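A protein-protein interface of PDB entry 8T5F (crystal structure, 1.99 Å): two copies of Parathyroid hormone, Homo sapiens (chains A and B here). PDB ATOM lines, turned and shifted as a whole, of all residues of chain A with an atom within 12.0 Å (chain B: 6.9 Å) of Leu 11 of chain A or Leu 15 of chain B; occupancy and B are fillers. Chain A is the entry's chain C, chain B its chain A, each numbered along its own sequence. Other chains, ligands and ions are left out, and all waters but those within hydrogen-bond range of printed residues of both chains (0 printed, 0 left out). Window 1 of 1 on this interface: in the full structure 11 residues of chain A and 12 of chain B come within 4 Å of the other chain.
Gln 6 of chain A touches none of the printed residues of chain B.
Printed residues of chain B within 4 Å of Met 8 of chain A: Met 18 (3.9 Å) and Glu 19 (3.6 Å).
Printed residues of chain B within 4 Å of His 9 of chain A: Glu 19.
Printed residues of chain B within 4 Å of Leu 11 of chain A: Leu 15.
Printed residues of chain B within 4 Å of Leu 15 of chain A: Leu 11 (3.8 Å) and Gly 12 (3.5 Å).
Printed residues of chain A within 4 Å of Leu 15 of chain B: Leu 11 (3.99 Å).
No residue of chain A comes within 4 Å of Ser 17 of chain B.
Met 18 of chain B touches just one residue of chain A: Met 8 (3.9 Å).
Of chain A, only Met 8 (3.6 Å) and His 9 (3.1 Å) come within 4 Å of Glu 19 of chain B.
The nearest printed residue of chain B that does not touch Leu 11 of chain A is Glu 19 of chain B (7.1 Å).
SD of Met 8 of chain A sits close to N of Glu 19 of chain B (3.7 Å).
A ring nitrogen (ND1) of His 9 of chain A is in hydrogen-bond range of the side-chain carboxylate (OE1) of Glu 19 of chain B (3.1 Å).
Of the 11 printed residues of chain B, 5 touch a printed residue of chain A.
Printed residues of chain B that touch a printed residue of chain A: Leu 11, Gly 12, Leu 15, Met 18 and Glu 19.
Hydrophobic or aromatic side chains of chain B within 4 Å of the printed part of chain A: Leu 11 and Leu 15.
Printed residues of chain A that touch a printed residue of chain B: Met 8, His 9, Leu 11 and Leu 15.
Hydrophobic or aromatic side chains of chain A within 4 Å of the printed part of chain B: Met 8, His 9, Leu 11 and Leu 15.
Among the printed residues, 6 pairs touch across the chains.
Leu 11 of chain A touches Leu 15 of chain B, and with the chains exchanged Leu 15 of chain A touches Leu 11 of chain B.
Leu 15 of chain A touches Gly 12 of chain B, but with the chains exchanged Gly 12 of chain A does not touch Leu 15 of chain B (4.1 Å).
Positions printed for both chains: 10, 11, 12, 13, 14, 15, 16, 17, 18, 19 and 20.
Met 8 of chain A touches Met 18 of chain B.
Leu 11 of chain A touches Leu 15 of chain B (CB to CD1, 3.99 Å).
CG of Leu 11 of chain B touches CD2 of Leu 15 of chain A (3.8 Å).
Leu 15 of chain A touches Gly 12 of chain B.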
ATOM      1  N   SER A   1      25.043 -35.640 -20.410  1.00  0.00           N
ATOM      2  CA  SER A   1      25.484 -35.416 -19.036  1.00  0.00           C
ATOM      3  C   SER A   1      24.854 -34.143 -18.448  1.00  0.00           C
ATOM      4  O   SER A   1      24.835 -33.088 -19.103  1.00  0.00           O
ATOM      5  CB  SER A   1      27.018 -35.334 -18.976  1.00  0.00           C
ATOM      6  OG  SER A   1      27.479 -34.855 -17.717  1.00  0.00           O
ATOM      7  N   VAL A   2      24.324 -34.259 -17.222  1.00  0.00           N
ATOM      8  CA  VAL A   2      23.848 -33.093 -16.470  1.00  0.00           C
ATOM      9  C   VAL A   2      25.014 -32.323 -15.826  1.00  0.00           C
ATOM     10  O   VAL A   2      24.858 -31.142 -15.475  1.00  0.00           O
ATOM     11  CB  VAL A   2      22.795 -33.534 -15.426  1.00  0.00           C
ATOM     12  CG1 VAL A   2      22.004 -32.343 -14.874  1.00  0.00           C
ATOM     13  CG2 VAL A   2      21.840 -34.566 -16.021  1.00  0.00           C
ATOM     14  N   SER A   3      26.185 -32.957 -15.666  1.00  0.00           N
ATOM     15  CA  SER A   3      27.385 -32.212 -15.304  1.00  0.00           C
ATOM     16  C   SER A   3      27.870 -31.348 -16.459  1.00  0.00           C
ATOM     17  O   SER A   3      28.525 -30.325 -16.231  1.00  0.00           O
ATOM     18  CB  SER A   3      28.506 -33.152 -14.862  1.00  0.00           C
ATOM     19  OG  SER A   3      29.338 -32.519 -13.896  1.00  0.00           O
ATOM     20  N   GLU A   4      27.584 -31.752 -17.698  1.00  0.00           N
ATOM     21  CA  GLU A   4      27.800 -30.856 -18.825  1.00  0.00           C
ATOM     22  C   GLU A   4      26.847 -29.665 -18.758  1.00  0.00           C
ATOM     23  O   GLU A   4      27.253 -28.531 -19.043  1.00  0.00           O
ATOM     24  CB  GLU A   4      27.619 -31.613 -20.137  1.00  0.00           C
ATOM     25  CG  GLU A   4      28.247 -30.972 -21.346  1.00  0.00           C
ATOM     26  CD  GLU A   4      28.030 -31.811 -22.595  1.00  0.00           C
ATOM     27  OE1 GLU A   4      28.218 -31.293 -23.726  1.00  0.00           O
ATOM     28  OE2 GLU A   4      27.607 -32.982 -22.433  1.00  0.00           O
ATOM     29  N   ILE A   5      25.578 -29.891 -18.390  1.00  0.00           N
ATOM     30  CA  ILE A   5      24.632 -28.777 -18.285  1.00  0.00           C
ATOM     31  C   ILE A   5      25.057 -27.823 -17.174  1.00  0.00           C
ATOM     32  O   ILE A   5      24.946 -26.595 -17.317  1.00  0.00           O
ATOM     33  CB  ILE A   5      23.187 -29.282 -18.075  1.00  0.00           C
ATOM     34  CG1 ILE A   5      22.538 -29.669 -19.394  1.00  0.00           C
ATOM     35  CG2 ILE A   5      22.307 -28.228 -17.450  1.00  0.00           C
ATOM     36  CD1 ILE A   5      21.455 -30.709 -19.244  1.00  0.00           C
ATOM     37  N   GLN A   6      25.579 -28.367 -16.073  1.00  0.00           N
ATOM     38  CA  GLN A   6      26.024 -27.550 -14.946  1.00  0.00           C
ATOM     39  C   GLN A   6      27.177 -26.627 -15.343  1.00  0.00           C
ATOM     40  O   GLN A   6      27.119 -25.416 -15.109  1.00  0.00           O
ATOM     41  CB  GLN A   6      26.439 -28.461 -13.798  1.00  0.00           C
ATOM     42  CG  GLN A   6      25.269 -28.956 -12.989  1.00  0.00           C
ATOM     43  CD  GLN A   6      25.703 -29.868 -11.862  1.00  0.00           C
ATOM     44  OE1 GLN A   6      26.819 -30.406 -11.876  1.00  0.00           O
ATOM     45  NE2 GLN A   6      24.852 -30.003 -10.851  1.00  0.00           N
ATOM     46  N   LEU A   7      28.239 -27.201 -15.926  1.00  0.00           N
ATOM     47  CA  LEU A   7      29.345 -26.427 -16.479  1.00  0.00           C
ATOM     48  C   LEU A   7      28.856 -25.316 -17.398  1.00  0.00           C
ATOM     49  O   LEU A   7      29.140 -24.131 -17.162  1.00  0.00           O
ATOM     50  CB  LEU A   7      30.287 -27.350 -17.249  1.00  0.00           C
ATOM     51  CG  LEU A   7      31.518 -26.630 -17.797  1.00  0.00           C
ATOM     52  CD1 LEU A   7      32.271 -25.939 -16.663  1.00  0.00           C
ATOM     53  CD2 LEU A   7      32.424 -27.564 -18.577  1.00  0.00           C
ATOM     54  N   MET A   8      28.141 -25.692 -18.472  1.00  0.00           N
ATOM     55  CA  MET A   8      27.594 -24.717 -19.415  1.00  0.00           C
ATOM     56  C   MET A   8      26.841 -23.616 -18.704  1.00  0.00           C
ATOM     57  O   MET A   8      27.026 -22.432 -19.002  1.00  0.00           O
ATOM     58  CB  MET A   8      26.672 -25.409 -20.431  1.00  0.00           C
ATOM     59  CG  MET A   8      27.394 -26.342 -21.388  1.00  0.00           C
ATOM     60  SD  MET A   8      26.211 -27.036 -22.567  1.00  0.00           S
ATOM     61  CE  MET A   8      27.171 -28.347 -23.325  1.00  0.00           C
ATOM     62  N   HIS A   9      25.968 -23.986 -17.781  1.00  0.00           N
ATOM     63  CA  HIS A   9      25.215 -22.985 -17.043  1.00  0.00           C
ATOM     64  C   HIS A   9      26.132 -22.074 -16.227  1.00  0.00           C
ATOM     65  O   HIS A   9      25.949 -20.847 -16.206  1.00  0.00           O
ATOM     66  CB  HIS A   9      24.201 -23.678 -16.143  1.00  0.00           C
ATOM     67  CG  HIS A   9      23.214 -22.733 -15.543  1.00  0.00           C
ATOM     68  ND1 HIS A   9      22.135 -22.247 -16.256  1.00  0.00           N
ATOM     69  CD2 HIS A   9      23.159 -22.149 -14.321  1.00  0.00           C
ATOM     70  CE1 HIS A   9      21.449 -21.417 -15.490  1.00  0.00           C
ATOM     71  NE2 HIS A   9      22.045 -21.343 -14.311  1.00  0.00           N
ATOM     72  N   ASN A  10      27.135 -22.644 -15.555  1.00  0.00           N
ATOM     73  CA  ASN A  10      28.016 -21.806 -14.743  1.00  0.00           C
ATOM     74  C   ASN A  10      28.890 -20.895 -15.617  1.00  0.00           C
ATOM     75  O   ASN A  10      29.163 -19.748 -15.246  1.00  0.00           O
ATOM     76  CB  ASN A  10      28.899 -22.670 -13.842  1.00  0.00           C
ATOM     77  CG  ASN A  10      29.734 -21.839 -12.912  1.00  0.00           C
ATOM     78  OD1 ASN A  10      30.914 -21.601 -13.152  1.00  0.00           O
ATOM     79  ND2 ASN A  10      29.120 -21.388 -11.823  1.00  0.00           N
ATOM     80  N   LEU A  11      29.338 -21.387 -16.776  1.00  0.00           N
ATOM     81  CA  LEU A  11      30.086 -20.555 -17.720  1.00  0.00           C
ATOM     82  C   LEU A  11      29.231 -19.399 -18.214  1.00  0.00           C
ATOM     83  O   LEU A  11      29.732 -18.275 -18.346  1.00  0.00           O
ATOM     84  CB  LEU A  11      30.539 -21.416 -18.895  1.00  0.00           C
ATOM     85  CG  LEU A  11      31.711 -22.332 -18.561  1.00  0.00           C
ATOM     86  CD1 LEU A  11      32.034 -23.255 -19.772  1.00  0.00           C
ATOM     87  CD2 LEU A  11      32.932 -21.524 -18.197  1.00  0.00           C
ATOM     88  N   GLY A  12      27.951 -19.669 -18.536  1.00  0.00           N
ATOM     89  CA  GLY A  12      27.014 -18.611 -18.926  1.00  0.00           C
ATOM     90  C   GLY A  12      26.844 -17.543 -17.847  1.00  0.00           C
ATOM     91  O   GLY A  12      26.796 -16.346 -18.147  1.00  0.00           O
ATOM     92  N   LYS A  13      26.745 -17.962 -16.584  1.00  0.00           N
ATOM     93  CA  LYS A  13      26.689 -17.008 -15.470  1.00  0.00           C
ATOM     94  C   LYS A  13      27.960 -16.177 -15.344  1.00  0.00           C
ATOM     95  O   LYS A  13      27.874 -14.969 -15.078  1.00  0.00           O
ATOM     96  CB  LYS A  13      26.394 -17.737 -14.153  1.00  0.00           C
ATOM     97  CG  LYS A  13      24.942 -18.227 -14.068  1.00  0.00           C
ATOM     98  CD  LYS A  13      24.436 -18.355 -12.616  1.00  0.00           C
ATOM     99  CE  LYS A  13      25.460 -19.019 -11.693  1.00  0.00           C
ATOM    100  NZ  LYS A  13      25.164 -20.479 -11.536  1.00  0.00           N
ATOM    101  N   HIS A  14      29.148 -16.798 -15.456  1.00  0.00           N
ATOM    102  CA  HIS A  14      30.385 -16.022 -15.477  1.00  0.00           C
ATOM    103  C   HIS A  14      30.378 -15.031 -16.637  1.00  0.00           C
ATOM    104  O   HIS A  14      30.778 -13.875 -16.488  1.00  0.00           O
ATOM    105  CB  HIS A  14      31.610 -16.952 -15.593  1.00  0.00           C
ATOM    106  CG  HIS A  14      32.079 -17.528 -14.287  1.00  0.00           C
ATOM    107  ND1 HIS A  14      32.597 -16.756 -13.270  1.00  0.00           N
ATOM    108  CD2 HIS A  14      32.083 -18.808 -13.825  1.00  0.00           C
ATOM    109  CE1 HIS A  14      32.923 -17.532 -12.247  1.00  0.00           C
ATOM    110  NE2 HIS A  14      32.623 -18.783 -12.558  1.00  0.00           N
ATOM    111  N   LEU A  15      29.954 -15.468 -17.815  1.00  0.00           N
ATOM    112  CA  LEU A  15      29.957 -14.565 -18.970  1.00  0.00           C
ATOM    113  C   LEU A  15      29.005 -13.386 -18.781  1.00  0.00           C
ATOM    114  O   LEU A  15      29.333 -12.248 -19.140  1.00  0.00           O
ATOM    115  CB  LEU A  15      29.580 -15.345 -20.230  1.00  0.00           C
ATOM    116  CG  LEU A  15      29.982 -14.731 -21.573  1.00  0.00           C
ATOM    117  CD1 LEU A  15      31.445 -14.226 -21.651  1.00  0.00           C
ATOM    118  CD2 LEU A  15      29.739 -15.735 -22.644  1.00  0.00           C
ATOM    119  N   ASN A  16      27.813 -13.635 -18.236  1.00  0.00           N
ATOM    120  CA  ASN A  16      26.892 -12.538 -17.919  1.00  0.00           C
ATOM    121  C   ASN A  16      27.510 -11.519 -16.962  1.00  0.00           C
ATOM    122  O   ASN A  16      27.278 -10.313 -17.131  1.00  0.00           O
ATOM    123  CB  ASN A  16      25.570 -13.062 -17.314  1.00  0.00           C
ATOM    124  CG  ASN A  16      24.622 -13.670 -18.339  1.00  0.00           C
ATOM    125  OD1 ASN A  16      24.873 -13.669 -19.552  1.00  0.00           O
ATOM    126  ND2 ASN A  16      23.524 -14.230 -17.841  1.00  0.00           N
ATOM    127  N   SER A  17      28.257 -11.969 -15.917  1.00  0.00           N
ATOM    128  CA  SER A  17      28.930 -10.995 -15.042  1.00  0.00           C
ATOM    129  C   SER A  17      30.023 -10.241 -15.774  1.00  0.00           C
ATOM    130  O   SER A  17      30.198  -9.033 -15.553  1.00  0.00           O
ATOM    131  CB  SER A  17      29.537 -11.651 -13.790  1.00  0.00           C
ATOM    132  OG  SER A  17      28.548 -12.407 -13.139  1.00  0.00           O
ATOM    133  N   MET A  18      30.803 -10.939 -16.619  1.00  0.00           N
ATOM    134  CA  MET A  18      31.817 -10.262 -17.425  1.00  0.00           C
ATOM    135  C   MET A  18      31.235  -9.178 -18.323  1.00  0.00           C
ATOM    136  O   MET A  18      31.864  -8.131 -18.495  1.00  0.00           O
ATOM    137  CB  MET A  18      32.645 -11.270 -18.242  1.00  0.00           C
ATOM    138  CG  MET A  18      33.263 -12.298 -17.317  1.00  0.00           C
ATOM    139  SD  MET A  18      33.980 -13.709 -18.183  1.00  0.00           S
ATOM    140  CE  MET A  18      35.276 -12.910 -19.147  1.00  0.00           C
ATOM    141  N   GLU A  19      30.047  -9.408 -18.902  1.00  0.00           N
ATOM    142  CA  GLU A  19      29.418  -8.411 -19.774  1.00  0.00           C
ATOM    143  C   GLU A  19      28.917  -7.219 -18.981  1.00  0.00           C
ATOM    144  O   GLU A  19      29.032  -6.068 -19.435  1.00  0.00           O
ATOM    145  CB  GLU A  19      28.234  -9.037 -20.535  1.00  0.00           C
ATOM    146  CG  GLU A  19      28.628 -10.211 -21.397  1.00  0.00           C
ATOM    147  CD  GLU A  19      27.416 -11.034 -21.905  1.00  0.00           C
ATOM    148  OE1 GLU A  19      27.635 -11.895 -22.774  1.00  0.00           O
ATOM    149  OE2 GLU A  19      26.269 -10.871 -21.412  1.00  0.00           O
ATOM    150  N   ARG A  20      28.313  -7.469 -17.821  1.00  0.00           N
ATOM    151  CA  ARG A  20      27.835  -6.372 -16.985  1.00  0.00           C
ATOM    152  C   ARG A  20      28.987  -5.502 -16.522  1.00  0.00           C
ATOM    153  O   ARG A  20      28.909  -4.263 -16.567  1.00  0.00           O
ATOM    154  CB  ARG A  20      27.065  -6.939 -15.795  1.00  0.00           C
ATOM    155  CG  ARG A  20      25.623  -7.259 -16.193  1.00  0.00           C
ATOM    156  CD  ARG A  20      25.065  -8.364 -15.330  1.00  0.00           C
ATOM    157  NE  ARG A  20      23.785  -8.857 -15.839  1.00  0.00           N
ATOM    158  CZ  ARG A  20      23.163  -9.940 -15.385  1.00  0.00           C
ATOM    159  NH1 ARG A  20      23.703 -10.713 -14.453  1.00  0.00           N
ATOM    160  NH2 ARG A  20      21.975 -10.266 -15.888  1.00  0.00           N
ATOM    161  N   ASN B  10      27.885 -12.888 -28.434  1.00  0.00           N
ATOM    162  CA  ASN B  10      27.891 -13.944 -29.458  1.00  0.00           C
ATOM    163  C   ASN B  10      28.397 -15.267 -28.898  1.00  0.00           C
ATOM    164  O   ASN B  10      27.838 -16.338 -29.179  1.00  0.00           O
ATOM    165  CB  ASN B  10      28.755 -13.527 -30.650  1.00  0.00           C
ATOM    166  CG  ASN B  10      28.181 -12.348 -31.394  1.00  0.00           C
ATOM    167  OD1 ASN B  10      26.987 -12.033 -31.262  1.00  0.00           O
ATOM    168  ND2 ASN B  10      29.007 -11.715 -32.221  1.00  0.00           N
ATOM    169  N   LEU B  11      29.434 -15.211 -28.079  1.00  0.00           N
ATOM    170  CA  LEU B  11      29.866 -16.414 -27.359  1.00  0.00           C
ATOM    171  C   LEU B  11      28.733 -16.946 -26.493  1.00  0.00           C
ATOM    172  O   LEU B  11      28.420 -18.149 -26.523  1.00  0.00           O
ATOM    173  CB  LEU B  11      31.131 -16.087 -26.538  1.00  0.00           C
ATOM    174  CG  LEU B  11      31.650 -17.210 -25.610  1.00  0.00           C
ATOM    175  CD1 LEU B  11      31.928 -18.441 -26.408  1.00  0.00           C
ATOM    176  CD2 LEU B  11      32.922 -16.811 -24.898  1.00  0.00           C
ATOM    177  N   GLY B  12      28.071 -16.063 -25.735  1.00  0.00           N
ATOM    178  CA  GLY B  12      26.994 -16.481 -24.846  1.00  0.00           C
ATOM    179  C   GLY B  12      25.821 -17.130 -25.565  1.00  0.00           C
ATOM    180  O   GLY B  12      25.182 -18.030 -25.010  1.00  0.00           O
ATOM    181  N   LYS B  13      25.504 -16.648 -26.774  1.00  0.00           N
ATOM    182  CA  LYS B  13      24.436 -17.235 -27.592  1.00  0.00           C
ATOM    183  C   LYS B  13      24.785 -18.660 -28.002  1.00  0.00           C
ATOM    184  O   LYS B  13      23.933 -19.555 -27.962  1.00  0.00           O
ATOM    185  CB  LYS B  13      24.212 -16.389 -28.858  1.00  0.00           C
ATOM    186  CG  LYS B  13      23.179 -16.997 -29.819  1.00  0.00           C
ATOM    187  CD  LYS B  13      23.733 -17.119 -31.256  1.00  0.00           C
ATOM    188  CE  LYS B  13      23.890 -15.780 -31.962  1.00  0.00           C
ATOM    189  NZ  LYS B  13      23.653 -15.910 -33.431  1.00  0.00           N
ATOM    190  N   HIS B  14      26.024 -18.868 -28.466  1.00  0.00           N
ATOM    191  CA  HIS B  14      26.487 -20.214 -28.825  1.00  0.00           C
ATOM    192  C   HIS B  14      26.400 -21.150 -27.628  1.00  0.00           C
ATOM    193  O   HIS B  14      25.936 -22.288 -27.735  1.00  0.00           O
ATOM    194  CB  HIS B  14      27.935 -20.157 -29.328  1.00  0.00           C
ATOM    195  CG  HIS B  14      28.122 -19.424 -30.621  1.00  0.00           C
ATOM    196  ND1 HIS B  14      27.099 -19.228 -31.530  1.00  0.00           N
ATOM    197  CD2 HIS B  14      29.231 -18.881 -31.187  1.00  0.00           C
ATOM    198  CE1 HIS B  14      27.563 -18.605 -32.599  1.00  0.00           C
ATOM    199  NE2 HIS B  14      28.853 -18.363 -32.409  1.00  0.00           N
ATOM    200  N   LEU B  15      26.897 -20.697 -26.491  1.00  0.00           N
ATOM    201  CA  LEU B  15      26.854 -21.474 -25.263  1.00  0.00           C
ATOM    202  C   LEU B  15      25.422 -21.807 -24.884  1.00  0.00           C
ATOM    203  O   LEU B  15      25.125 -22.917 -24.421  1.00  0.00           O
ATOM    204  CB  LEU B  15      27.501 -20.652 -24.145  1.00  0.00           C
ATOM    205  CG  LEU B  15      28.992 -20.722 -23.823  1.00  0.00           C
ATOM    206  CD1 LEU B  15      29.215 -20.112 -22.430  1.00  0.00           C
ATOM    207  CD2 LEU B  15      29.533 -22.170 -23.884  1.00  0.00           C
ATOM    208  N   ASN B  16      24.533 -20.827 -25.002  1.00  0.00           N
ATOM    209  CA  ASN B  16      23.141 -21.029 -24.655  1.00  0.00           C
ATOM    210  C   ASN B  16      22.473 -22.016 -25.612  1.00  0.00           C
ATOM    211  O   ASN B  16      21.620 -22.805 -25.190  1.00  0.00           O
ATOM    212  CB  ASN B  16      22.413 -19.683 -24.691  1.00  0.00           C
ATOM    213  CG  ASN B  16      20.936 -19.812 -24.348  1.00  0.00           C
ATOM    214  OD1 ASN B  16      20.053 -19.770 -25.222  1.00  0.00           O
ATOM    215  ND2 ASN B  16      20.659 -19.973 -23.074  1.00  0.00           N
ATOM    216  N   SER B  17      22.844 -21.974 -26.893  1.00  0.00           N
ATOM    217  CA  SER B  17      22.318 -22.925 -27.870  1.00  0.00           C
ATOM    218  C   SER B  17      22.739 -24.349 -27.544  1.00  0.00           C
ATOM    219  O   SER B  17      21.908 -25.270 -27.550  1.00  0.00           O
ATOM    220  CB  SER B  17      22.790 -22.535 -29.265  1.00  0.00           C
ATOM    221  OG  SER B  17      22.115 -21.357 -29.628  1.00  0.00           O
ATOM    222  N   MET B  18      24.015 -24.547 -27.210  1.00  0.00           N
ATOM    223  CA  MET B  18      24.470 -25.871 -26.787  1.00  0.00           C
ATOM    224  C   MET B  18      23.755 -26.334 -25.531  1.00  0.00           C
ATOM    225  O   MET B  18      23.414 -27.519 -25.406  1.00  0.00           O
ATOM    226  CB  MET B  18      25.984 -25.855 -26.562  1.00  0.00           C
ATOM    227  CG  MET B  18      26.765 -25.620 -27.852  1.00  0.00           C
ATOM    228  SD  MET B  18      28.582 -25.640 -27.651  1.00  0.00           S
ATOM    229  CE  MET B  18      28.937 -23.911 -27.494  1.00  0.00           C
ATOM    230  N   GLU B  19      23.560 -25.420 -24.569  1.00  0.00           N
ATOM    231  CA  GLU B  19      22.882 -25.759 -23.317  1.00  0.00           C
ATOM    232  C   GLU B  19      21.447 -26.220 -23.543  1.00  0.00           C
ATOM    233  O   GLU B  19      20.951 -27.091 -22.817  1.00  0.00           O
ATOM    234  CB  GLU B  19      22.887 -24.548 -22.371  1.00  0.00           C
ATOM    235  CG  GLU B  19      22.344 -24.867 -21.010  1.00  0.00           C
ATOM    236  CD  GLU B  19      22.564 -23.754 -19.998  1.00  0.00           C
ATOM    237  OE1 GLU B  19      21.959 -23.856 -18.903  1.00  0.00           O
ATOM    238  OE2 GLU B  19      23.340 -22.807 -20.279  1.00  0.00           O
ATOM    239  N   ARG B  20      20.742 -25.595 -24.494  1.00  0.00           N
ATOM    240  CA  ARG B  20      19.352 -25.939 -24.768  1.00  0.00           C
ATOM    241  C   ARG B  20      19.241 -27.317 -25.393  1.00  0.00           C
ATOM    242  O   ARG B  20      18.283 -28.054 -25.127  1.00  0.00           O
ATOM    243  CB  ARG B  20      18.744 -24.885 -25.691  1.00  0.00           C
ATOM    244  CG  ARG B  20      18.199 -23.695 -24.926  1.00  0.00           C
ATOM    245  CD  ARG B  20      17.781 -22.564 -25.840  1.00  0.00           C
ATOM    246  NE  ARG B  20      17.410 -21.339 -25.129  1.00  0.00           N
ATOM    247  CZ  ARG B  20      16.250 -21.137 -24.505  1.00  0.00           C
ATOM    248  NH1 ARG B  20      15.311 -22.073 -24.457  1.00  0.00           N
ATOM    249  NH2 ARG B  20      16.023 -19.963 -23.921  1.00  0.00           N
